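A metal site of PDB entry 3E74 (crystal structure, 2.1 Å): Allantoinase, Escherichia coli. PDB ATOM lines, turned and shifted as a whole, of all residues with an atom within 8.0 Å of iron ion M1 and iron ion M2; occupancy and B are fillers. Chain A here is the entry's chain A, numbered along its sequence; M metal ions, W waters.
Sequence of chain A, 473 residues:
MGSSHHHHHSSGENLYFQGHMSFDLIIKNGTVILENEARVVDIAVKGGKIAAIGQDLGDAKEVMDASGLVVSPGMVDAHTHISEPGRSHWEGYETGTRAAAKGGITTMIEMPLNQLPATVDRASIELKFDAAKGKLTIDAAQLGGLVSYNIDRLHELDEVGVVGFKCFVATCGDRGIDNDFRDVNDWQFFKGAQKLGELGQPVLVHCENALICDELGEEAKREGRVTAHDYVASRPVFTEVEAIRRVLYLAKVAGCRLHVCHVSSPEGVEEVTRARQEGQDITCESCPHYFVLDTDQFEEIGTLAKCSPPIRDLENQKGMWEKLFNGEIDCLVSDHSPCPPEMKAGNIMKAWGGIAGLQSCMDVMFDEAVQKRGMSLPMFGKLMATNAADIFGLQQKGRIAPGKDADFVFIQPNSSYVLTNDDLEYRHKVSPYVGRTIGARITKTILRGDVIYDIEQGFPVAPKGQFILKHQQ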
ATOM      1  N   HIS A  79       4.608   9.257   2.752  1.00  0.00           N
ATOM      2  CA  HIS A  79       6.057   9.166   2.789  1.00  0.00           C
ATOM      3  C   HIS A  79       6.715   9.171   1.410  1.00  0.00           C
ATOM      4  O   HIS A  79       7.131   8.134   0.881  1.00  0.00           O
ATOM      5  CB  HIS A  79       6.461   7.908   3.553  1.00  0.00           C
ATOM      6  CG  HIS A  79       7.913   7.847   3.902  1.00  0.00           C
ATOM      7  ND1 HIS A  79       8.388   7.168   5.001  1.00  0.00           N
ATOM      8  CD2 HIS A  79       8.999   8.371   3.281  1.00  0.00           C
ATOM      9  CE1 HIS A  79       9.704   7.265   5.043  1.00  0.00           C
ATOM     10  NE2 HIS A  79      10.106   7.987   3.999  1.00  0.00           N
ATOM     11  N   THR A  80       6.841  10.365   0.827  1.00  0.00           N
ATOM     12  CA  THR A  80       7.464  10.445  -0.473  1.00  0.00           C
ATOM     13  C   THR A  80       8.590  11.475  -0.573  1.00  0.00           C
ATOM     14  O   THR A  80       8.547  12.539   0.044  1.00  0.00           O
ATOM     15  CB  THR A  80       6.385  10.658  -1.586  1.00  0.00           C
ATOM     16  OG1 THR A  80       6.927  11.452  -2.645  1.00  0.00           O
ATOM     17  CG2 THR A  80       5.146  11.274  -1.027  1.00  0.00           C
ATOM     18  N   HIS A  81       9.617  11.111  -1.332  1.00  0.00           N
ATOM     19  CA  HIS A  81      10.772  11.985  -1.542  1.00  0.00           C
ATOM     20  C   HIS A  81      10.727  12.504  -2.975  1.00  0.00           C
ATOM     21  O   HIS A  81      10.640  11.731  -3.922  1.00  0.00           O
ATOM     22  CB  HIS A  81      12.061  11.220  -1.301  1.00  0.00           C
ATOM     23  CG  HIS A  81      12.195  10.694   0.107  1.00  0.00           C
ATOM     24  ND1 HIS A  81      12.605  11.481   1.159  1.00  0.00           N
ATOM     25  CD2 HIS A  81      11.935   9.471   0.619  1.00  0.00           C
ATOM     26  CE1 HIS A  81      12.590  10.760   2.272  1.00  0.00           C
ATOM     27  NE2 HIS A  81      12.182   9.544   1.971  1.00  0.00           N
ATOM     28  N   MET A 111       8.537  14.669   2.292  1.00  0.00           N
ATOM     29  CA  MET A 111       9.590  14.574   3.288  1.00  0.00           C
ATOM     30  C   MET A 111      10.465  15.814   3.212  1.00  0.00           C
ATOM     31  O   MET A 111      10.652  16.378   2.139  1.00  0.00           O
ATOM     32  CB  MET A 111      10.419  13.317   3.063  1.00  0.00           C
ATOM     33  CG  MET A 111       9.701  12.037   3.488  1.00  0.00           C
ATOM     34  SD  MET A 111       9.645  11.848   5.427  1.00  0.00           S
ATOM     35  CE  MET A 111       8.139  10.632   5.618  1.00  0.00           C
ATOM     36  N   LEU A 113      14.055  16.351   4.869  1.00  0.00           N
ATOM     37  CA  LEU A 113      15.488  16.170   4.696  1.00  0.00           C
ATOM     38  C   LEU A 113      15.878  15.607   3.327  1.00  0.00           C
ATOM     39  O   LEU A 113      15.003  15.269   2.529  1.00  0.00           O
ATOM     40  CB  LEU A 113      16.036  15.283   5.834  1.00  0.00           C
ATOM     41  CG  LEU A 113      16.196  15.962   7.208  1.00  0.00           C
ATOM     42  CD1 LEU A 113      14.864  16.492   7.686  1.00  0.00           C
ATOM     43  CD2 LEU A 113      16.738  14.967   8.212  1.00  0.00           C
ATOM     44  N   ASN A 114      17.184  15.542   3.078  1.00  0.00           N
ATOM     45  CA  ASN A 114      17.721  15.044   1.811  1.00  0.00           C
ATOM     46  C   ASN A 114      17.093  15.753   0.611  1.00  0.00           C
ATOM     47  O   ASN A 114      16.506  15.133  -0.279  1.00  0.00           O
ATOM     48  CB  ASN A 114      17.514  13.528   1.693  1.00  0.00           C
ATOM     49  CG  ASN A 114      18.377  12.748   2.670  1.00  0.00           C
ATOM     50  OD1 ASN A 114      19.609  12.740   2.559  1.00  0.00           O
ATOM     51  ND2 ASN A 114      17.744  12.112   3.655  1.00  0.00           N
ATOM     52  N   KCX A 166       9.837  15.066  10.500  1.00  0.00           N
ATOM     53  CA  KCX A 166      10.646  13.869  10.331  1.00  0.00           C
ATOM     54  CB  KCX A 166      10.786  13.553   8.848  1.00  0.00           C
ATOM     55  CG  KCX A 166      10.711  12.090   8.466  1.00  0.00           C
ATOM     56  CD  KCX A 166      11.860  11.280   8.993  1.00  0.00           C
ATOM     57  CE  KCX A 166      11.889   9.885   8.372  1.00  0.00           C
ATOM     58  NZ  KCX A 166      12.188   9.912   6.933  1.00  0.00           N
ATOM     59  C   KCX A 166      12.041  14.044  10.951  1.00  0.00           C
ATOM     60  O   KCX A 166      12.608  15.142  10.934  1.00  0.00           O
ATOM     61  CX  KCX A 166      12.682   8.885   6.240  1.00  0.00           C
ATOM     62  OQ1 KCX A 166      12.898   9.025   5.012  1.00  0.00           O
ATOM     63  OQ2 KCX A 166      12.933   7.811   6.845  1.00  0.00           O
ATOM     64  N   CYS A 167      12.591  12.951  11.495  1.00  0.00           N
ATOM     65  CA  CYS A 167      13.930  12.979  12.070  1.00  0.00           C
ATOM     66  C   CYS A 167      14.547  11.580  12.047  1.00  0.00           C
ATOM     67  O   CYS A 167      13.830  10.566  11.917  1.00  0.00           O
ATOM     68  CB  CYS A 167      13.911  13.505  13.500  1.00  0.00           C
ATOM     69  SG  CYS A 167      13.267  12.350  14.717  1.00  0.00           S
ATOM     70  N   PHE A 168      15.872  11.532  12.152  1.00  0.00           N
ATOM     71  CA  PHE A 168      16.580  10.269  12.146  1.00  0.00           C
ATOM     72  C   PHE A 168      17.286  10.029  13.459  1.00  0.00           C
ATOM     73  O   PHE A 168      18.035  10.890  13.946  1.00  0.00           O
ATOM     74  CB  PHE A 168      17.583  10.228  10.988  1.00  0.00           C
ATOM     75  CG  PHE A 168      16.959  10.342   9.637  1.00  0.00           C
ATOM     76  CD1 PHE A 168      16.404  11.545   9.208  1.00  0.00           C
ATOM     77  CD2 PHE A 168      16.851   9.220   8.811  1.00  0.00           C
ATOM     78  CE1 PHE A 168      15.748  11.634   7.979  1.00  0.00           C
ATOM     79  CE2 PHE A 168      16.193   9.307   7.573  1.00  0.00           C
ATOM     80  CZ  PHE A 168      15.646  10.505   7.153  1.00  0.00           C
ATOM     81  N   VAL A 205       9.658   9.044  12.743  1.00  0.00           N
ATOM     82  CA  VAL A 205      11.028   8.585  12.889  1.00  0.00           C
ATOM     83  C   VAL A 205      11.455   7.364  12.079  1.00  0.00           C
ATOM     84  O   VAL A 205      10.732   6.371  11.999  1.00  0.00           O
ATOM     85  CB  VAL A 205      11.369   8.261  14.382  1.00  0.00           C
ATOM     86  CG1 VAL A 205      12.840   7.959  14.515  1.00  0.00           C
ATOM     87  CG2 VAL A 205      10.967   9.400  15.310  1.00  0.00           C
ATOM     88  N   HIS A 206      12.658   7.472  11.500  1.00  0.00           N
ATOM     89  CA  HIS A 206      13.307   6.388  10.754  1.00  0.00           C
ATOM     90  C   HIS A 206      14.006   5.568  11.863  1.00  0.00           C
ATOM     91  O   HIS A 206      15.033   6.000  12.391  1.00  0.00           O
ATOM     92  CB  HIS A 206      14.372   6.959   9.797  1.00  0.00           C
ATOM     93  CG  HIS A 206      15.154   5.904   9.090  1.00  0.00           C
ATOM     94  ND1 HIS A 206      14.997   5.635   7.747  1.00  0.00           N
ATOM     95  CD2 HIS A 206      16.033   4.982   9.552  1.00  0.00           C
ATOM     96  CE1 HIS A 206      15.742   4.591   7.411  1.00  0.00           C
ATOM     97  NE2 HIS A 206      16.369   4.173   8.490  1.00  0.00           N
ATOM     98  N   CYS A 207      13.471   4.408  12.216  1.00  0.00           N
ATOM     99  CA  CYS A 207      14.036   3.635  13.322  1.00  0.00           C
ATOM    100  C   CYS A 207      14.959   2.451  13.042  1.00  0.00           C
ATOM    101  O   CYS A 207      14.491   1.315  12.889  1.00  0.00           O
ATOM    102  CB  CYS A 207      12.899   3.147  14.237  1.00  0.00           C
ATOM    103  SG  CYS A 207      11.823   4.440  14.889  1.00  0.00           S
ATOM    104  N   GLU A 208      16.261   2.716  13.016  1.00  0.00           N
ATOM    105  CA  GLU A 208      17.317   1.701  12.840  1.00  0.00           C
ATOM    106  C   GLU A 208      18.539   2.161  13.625  1.00  0.00           C
ATOM    107  O   GLU A 208      18.846   3.372  13.678  1.00  0.00           O
ATOM    108  CB  GLU A 208      17.769   1.581  11.391  1.00  0.00           C
ATOM    109  CG  GLU A 208      16.919   0.715  10.486  1.00  0.00           C
ATOM    110  CD  GLU A 208      17.550   0.571   9.118  1.00  0.00           C
ATOM    111  OE1 GLU A 208      17.797   1.604   8.462  1.00  0.00           O
ATOM    112  OE2 GLU A 208      17.801  -0.597   8.710  1.00  0.00           O
ATOM    113  N   CYS A 261       8.188   5.108  11.019  1.00  0.00           N
ATOM    114  CA  CYS A 261       8.370   4.966   9.569  1.00  0.00           C
ATOM    115  C   CYS A 261       8.771   3.573   9.074  1.00  0.00           C
ATOM    116  O   CYS A 261       9.395   2.769   9.796  1.00  0.00           O
ATOM    117  CB  CYS A 261       9.388   6.012   9.070  1.00  0.00           C
ATOM    118  SG  CYS A 261       8.748   7.736   8.980  1.00  0.00           S
ATOM    119  N   HIS A 262       8.346   3.284   7.846  1.00  0.00           N
ATOM    120  CA  HIS A 262       8.635   2.030   7.148  1.00  0.00           C
ATOM    121  C   HIS A 262       9.125   0.866   8.046  1.00  0.00           C
ATOM    122  O   HIS A 262      10.327   0.606   8.141  1.00  0.00           O
ATOM    123  CB  HIS A 262       9.663   2.329   6.062  1.00  0.00           C
ATOM    124  CG  HIS A 262      10.831   3.140   6.546  1.00  0.00           C
ATOM    125  ND1 HIS A 262      11.523   2.837   7.696  1.00  0.00           N
ATOM    126  CD2 HIS A 262      11.460   4.221   6.002  1.00  0.00           C
ATOM    127  CE1 HIS A 262      12.530   3.685   7.845  1.00  0.00           C
ATOM    128  NE2 HIS A 262      12.508   4.531   6.831  1.00  0.00           N
ATOM    129  N   GLU A 285       3.790   2.609   9.781  1.00  0.00           N
ATOM    130  CA  GLU A 285       3.524   2.367   8.367  1.00  0.00           C
ATOM    131  C   GLU A 285       4.511   1.323   7.854  1.00  0.00           C
ATOM    132  O   GLU A 285       5.431   0.931   8.564  1.00  0.00           O
ATOM    133  CB  GLU A 285       3.789   3.645   7.584  1.00  0.00           C
ATOM    134  CG  GLU A 285       5.262   4.083   7.746  1.00  0.00           C
ATOM    135  CD  GLU A 285       5.644   5.389   7.029  1.00  0.00           C
ATOM    136  OE1 GLU A 285       4.807   6.320   6.927  1.00  0.00           O
ATOM    137  OE2 GLU A 285       6.812   5.482   6.582  1.00  0.00           O
ATOM    138  N   CYS A 287       5.794  -0.382   3.641  1.00  0.00           N
ATOM    139  CA  CYS A 287       5.743  -0.096   2.211  1.00  0.00           C
ATOM    140  C   CYS A 287       5.521  -1.358   1.397  1.00  0.00           C
ATOM    141  O   CYS A 287       5.843  -2.453   1.859  1.00  0.00           O
ATOM    142  CB  CYS A 287       7.068   0.541   1.793  1.00  0.00           C
ATOM    143  SG  CYS A 287       7.680   1.744   2.987  1.00  0.00           S
ATOM    144  N   TYR A 290       8.041  -4.389   1.213  1.00  0.00           N
ATOM    145  CA  TYR A 290       8.221  -5.327   2.320  1.00  0.00           C
ATOM    146  C   TYR A 290       7.118  -6.402   2.306  1.00  0.00           C
ATOM    147  O   TYR A 290       7.183  -7.380   3.050  1.00  0.00           O
ATOM    148  CB  TYR A 290       8.185  -4.585   3.672  1.00  0.00           C
ATOM    149  CG  TYR A 290       9.262  -3.542   3.808  1.00  0.00           C
ATOM    150  CD1 TYR A 290      10.610  -3.891   3.860  1.00  0.00           C
ATOM    151  CD2 TYR A 290       8.928  -2.187   3.865  1.00  0.00           C
ATOM    152  CE1 TYR A 290      11.614  -2.905   3.976  1.00  0.00           C
ATOM    153  CE2 TYR A 290       9.906  -1.209   3.970  1.00  0.00           C
ATOM    154  CZ  TYR A 290      11.247  -1.564   4.025  1.00  0.00           C
ATOM    155  OH  TYR A 290      12.211  -0.585   4.102  1.00  0.00           O
ATOM    156  N   CYS A 307      17.214  -1.019  -0.127  1.00  0.00           N
ATOM    157  CA  CYS A 307      16.626   0.087   0.639  1.00  0.00           C
ATOM    158  C   CYS A 307      17.029  -0.021   2.106  1.00  0.00           C
ATOM    159  O   CYS A 307      17.385  -1.102   2.576  1.00  0.00           O
ATOM    160  CB  CYS A 307      15.107   0.098   0.524  1.00  0.00           C
ATOM    161  SG  CYS A 307      14.387  -1.477   0.943  1.00  0.00           S
ATOM    162  N   SER A 308      16.954   1.095   2.827  1.00  0.00           N
ATOM    163  CA  SER A 308      17.377   1.142   4.219  1.00  0.00           C
ATOM    164  C   SER A 308      16.812   0.035   5.082  1.00  0.00           C
ATOM    165  O   SER A 308      17.488  -0.985   5.241  1.00  0.00           O
ATOM    166  CB  SER A 308      17.096   2.502   4.826  1.00  0.00           C
ATOM    167  OG  SER A 308      18.038   2.754   5.848  1.00  0.00           O
ATOM    168  N   PRO A 309      15.613   0.199   5.692  1.00  0.00           N
ATOM    169  CA  PRO A 309      15.274  -1.022   6.440  1.00  0.00           C
ATOM    170  C   PRO A 309      15.281  -2.003   5.258  1.00  0.00           C
ATOM    171  O   PRO A 309      14.592  -1.761   4.271  1.00  0.00           O
ATOM    172  CB  PRO A 309      13.873  -0.738   6.995  1.00  0.00           C
ATOM    173  CG  PRO A 309      13.786   0.735   6.996  1.00  0.00           C
ATOM    174  CD  PRO A 309      14.490   1.146   5.701  1.00  0.00           C
ATOM    175  N   VAL A 333       2.861   3.198   2.642  1.00  0.00           N
ATOM    176  CA  VAL A 333       3.405   4.364   1.975  1.00  0.00           C
ATOM    177  C   VAL A 333       4.456   3.865   0.985  1.00  0.00           C
ATOM    178  O   VAL A 333       4.887   2.715   1.044  1.00  0.00           O
ATOM    179  CB  VAL A 333       4.030   5.373   2.988  1.00  0.00           C
ATOM    180  CG1 VAL A 333       2.958   5.854   3.988  1.00  0.00           C
ATOM    181  CG2 VAL A 333       5.192   4.739   3.748  1.00  0.00           C
ATOM    182  N   SER A 334       4.869   4.724   0.077  1.00  0.00           N
ATOM    183  CA  SER A 334       5.843   4.330  -0.927  1.00  0.00           C
ATOM    184  C   SER A 334       7.302   4.453  -0.516  1.00  0.00           C
ATOM    185  O   SER A 334       8.126   3.637  -0.907  1.00  0.00           O
ATOM    186  CB  SER A 334       5.640   5.198  -2.171  1.00  0.00           C
ATOM    187  OG  SER A 334       6.118   6.507  -1.912  1.00  0.00           O
ATOM    188  N   ASP A 335       7.623   5.461   0.286  1.00  0.00           N
ATOM    189  CA  ASP A 335       9.025   5.742   0.612  1.00  0.00           C
ATOM    190  C   ASP A 335       9.760   5.872  -0.743  1.00  0.00           C
ATOM    191  O   ASP A 335      10.922   5.464  -0.890  1.00  0.00           O
ATOM    192  CB  ASP A 335       9.707   4.654   1.469  1.00  0.00           C
ATOM    193  CG  ASP A 335      11.091   5.112   1.993  1.00  0.00           C
ATOM    194  OD1 ASP A 335      11.356   6.329   1.994  1.00  0.00           O
ATOM    195  OD2 ASP A 335      11.930   4.273   2.394  1.00  0.00           O
ATOM    196  N   HIS A 336       9.063   6.414  -1.735  1.00  0.00           N
ATOM    197  CA  HIS A 336       9.645   6.601  -3.059  1.00  0.00           C
ATOM    198  C   HIS A 336      10.969   7.317  -2.919  1.00  0.00           C
ATOM    199  O   HIS A 336      11.041   8.421  -2.366  1.00  0.00           O
ATOM    200  CB  HIS A 336       8.702   7.394  -3.952  1.00  0.00           C
ATOM    201  CG  HIS A 336       9.230   7.615  -5.332  1.00  0.00           C
ATOM    202  ND1 HIS A 336       9.548   6.576  -6.185  1.00  0.00           N
ATOM    203  CD2 HIS A 336       9.453   8.757  -6.028  1.00  0.00           C
ATOM    204  CE1 HIS A 336       9.936   7.069  -7.353  1.00  0.00           C
ATOM    205  NE2 HIS A 336       9.880   8.389  -7.283  1.00  0.00           N
ATOM    206  N   SER A 337      12.026   6.671  -3.396  1.00  0.00           N
ATOM    207  CA  SER A 337      13.360   7.229  -3.296  1.00  0.00           C
ATOM    208  C   SER A 337      14.149   6.943  -4.570  1.00  0.00           C
ATOM    209  O   SER A 337      14.892   5.962  -4.663  1.00  0.00           O
ATOM    210  CB  SER A 337      14.082   6.632  -2.086  1.00  0.00           C
ATOM    211  OG  SER A 337      15.363   7.225  -1.926  1.00  0.00           O
HETATM  212 FE    FE M   1      12.320   7.835   3.399  1.00  0.00          FE
HETATM  213 FE    FE M   2      13.969   6.242   5.908  1.00  0.00          FE
HETATM  214  O   HOH W   1      15.467   7.877   3.796  1.00  0.00           O
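Iron ion M1 is bound by OQ1 of KCX 166, NE2 of His 81, OD1 of Asp 335 and NE2 of His 79. Iron ion M1 has four donor atoms within binding distance.
O of His 336 sits close to N of His 81, 3.2 Å away. The backbone NH (N) of His 206 is in hydrogen-bond range of the backbone carbonyl oxygen (O) of Cys 167 (3.3 Å). O of His 79 sits at hydrogen-bond distance from OG of Ser 334. N of His 262 lies within hydrogen-bond range of OE2 of Glu 285. NZ of KCX 166 sits close to SD of Met 111 (3.5 Å). ND1 of His 79 sits at hydrogen-bond distance from OE2 of Glu 285, 2.8 Å away. A ring nitrogen (NE2) of His 206 lies within hydrogen-bond range of the side-chain carboxylate (OE1) of Glu 208, at 2.9 Å. NE2 of His 206 sits close to OG of Ser 308, at 3.4 Å.
Iron ion M2 is bound by OQ2 of KCX 166, ND1 of His 206 and NE2 of His 262. Iron ion M2 has three donor atoms within binding distance.
Within 4 Å of iron ion M2: KCX 166, His 206 and His 262.
Along chain A the residues within 4 Å of iron ion M1 span positions 79 to 335. The nearest printed residue that does not touch iron ion M1 is His 262 (4.5 Å).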
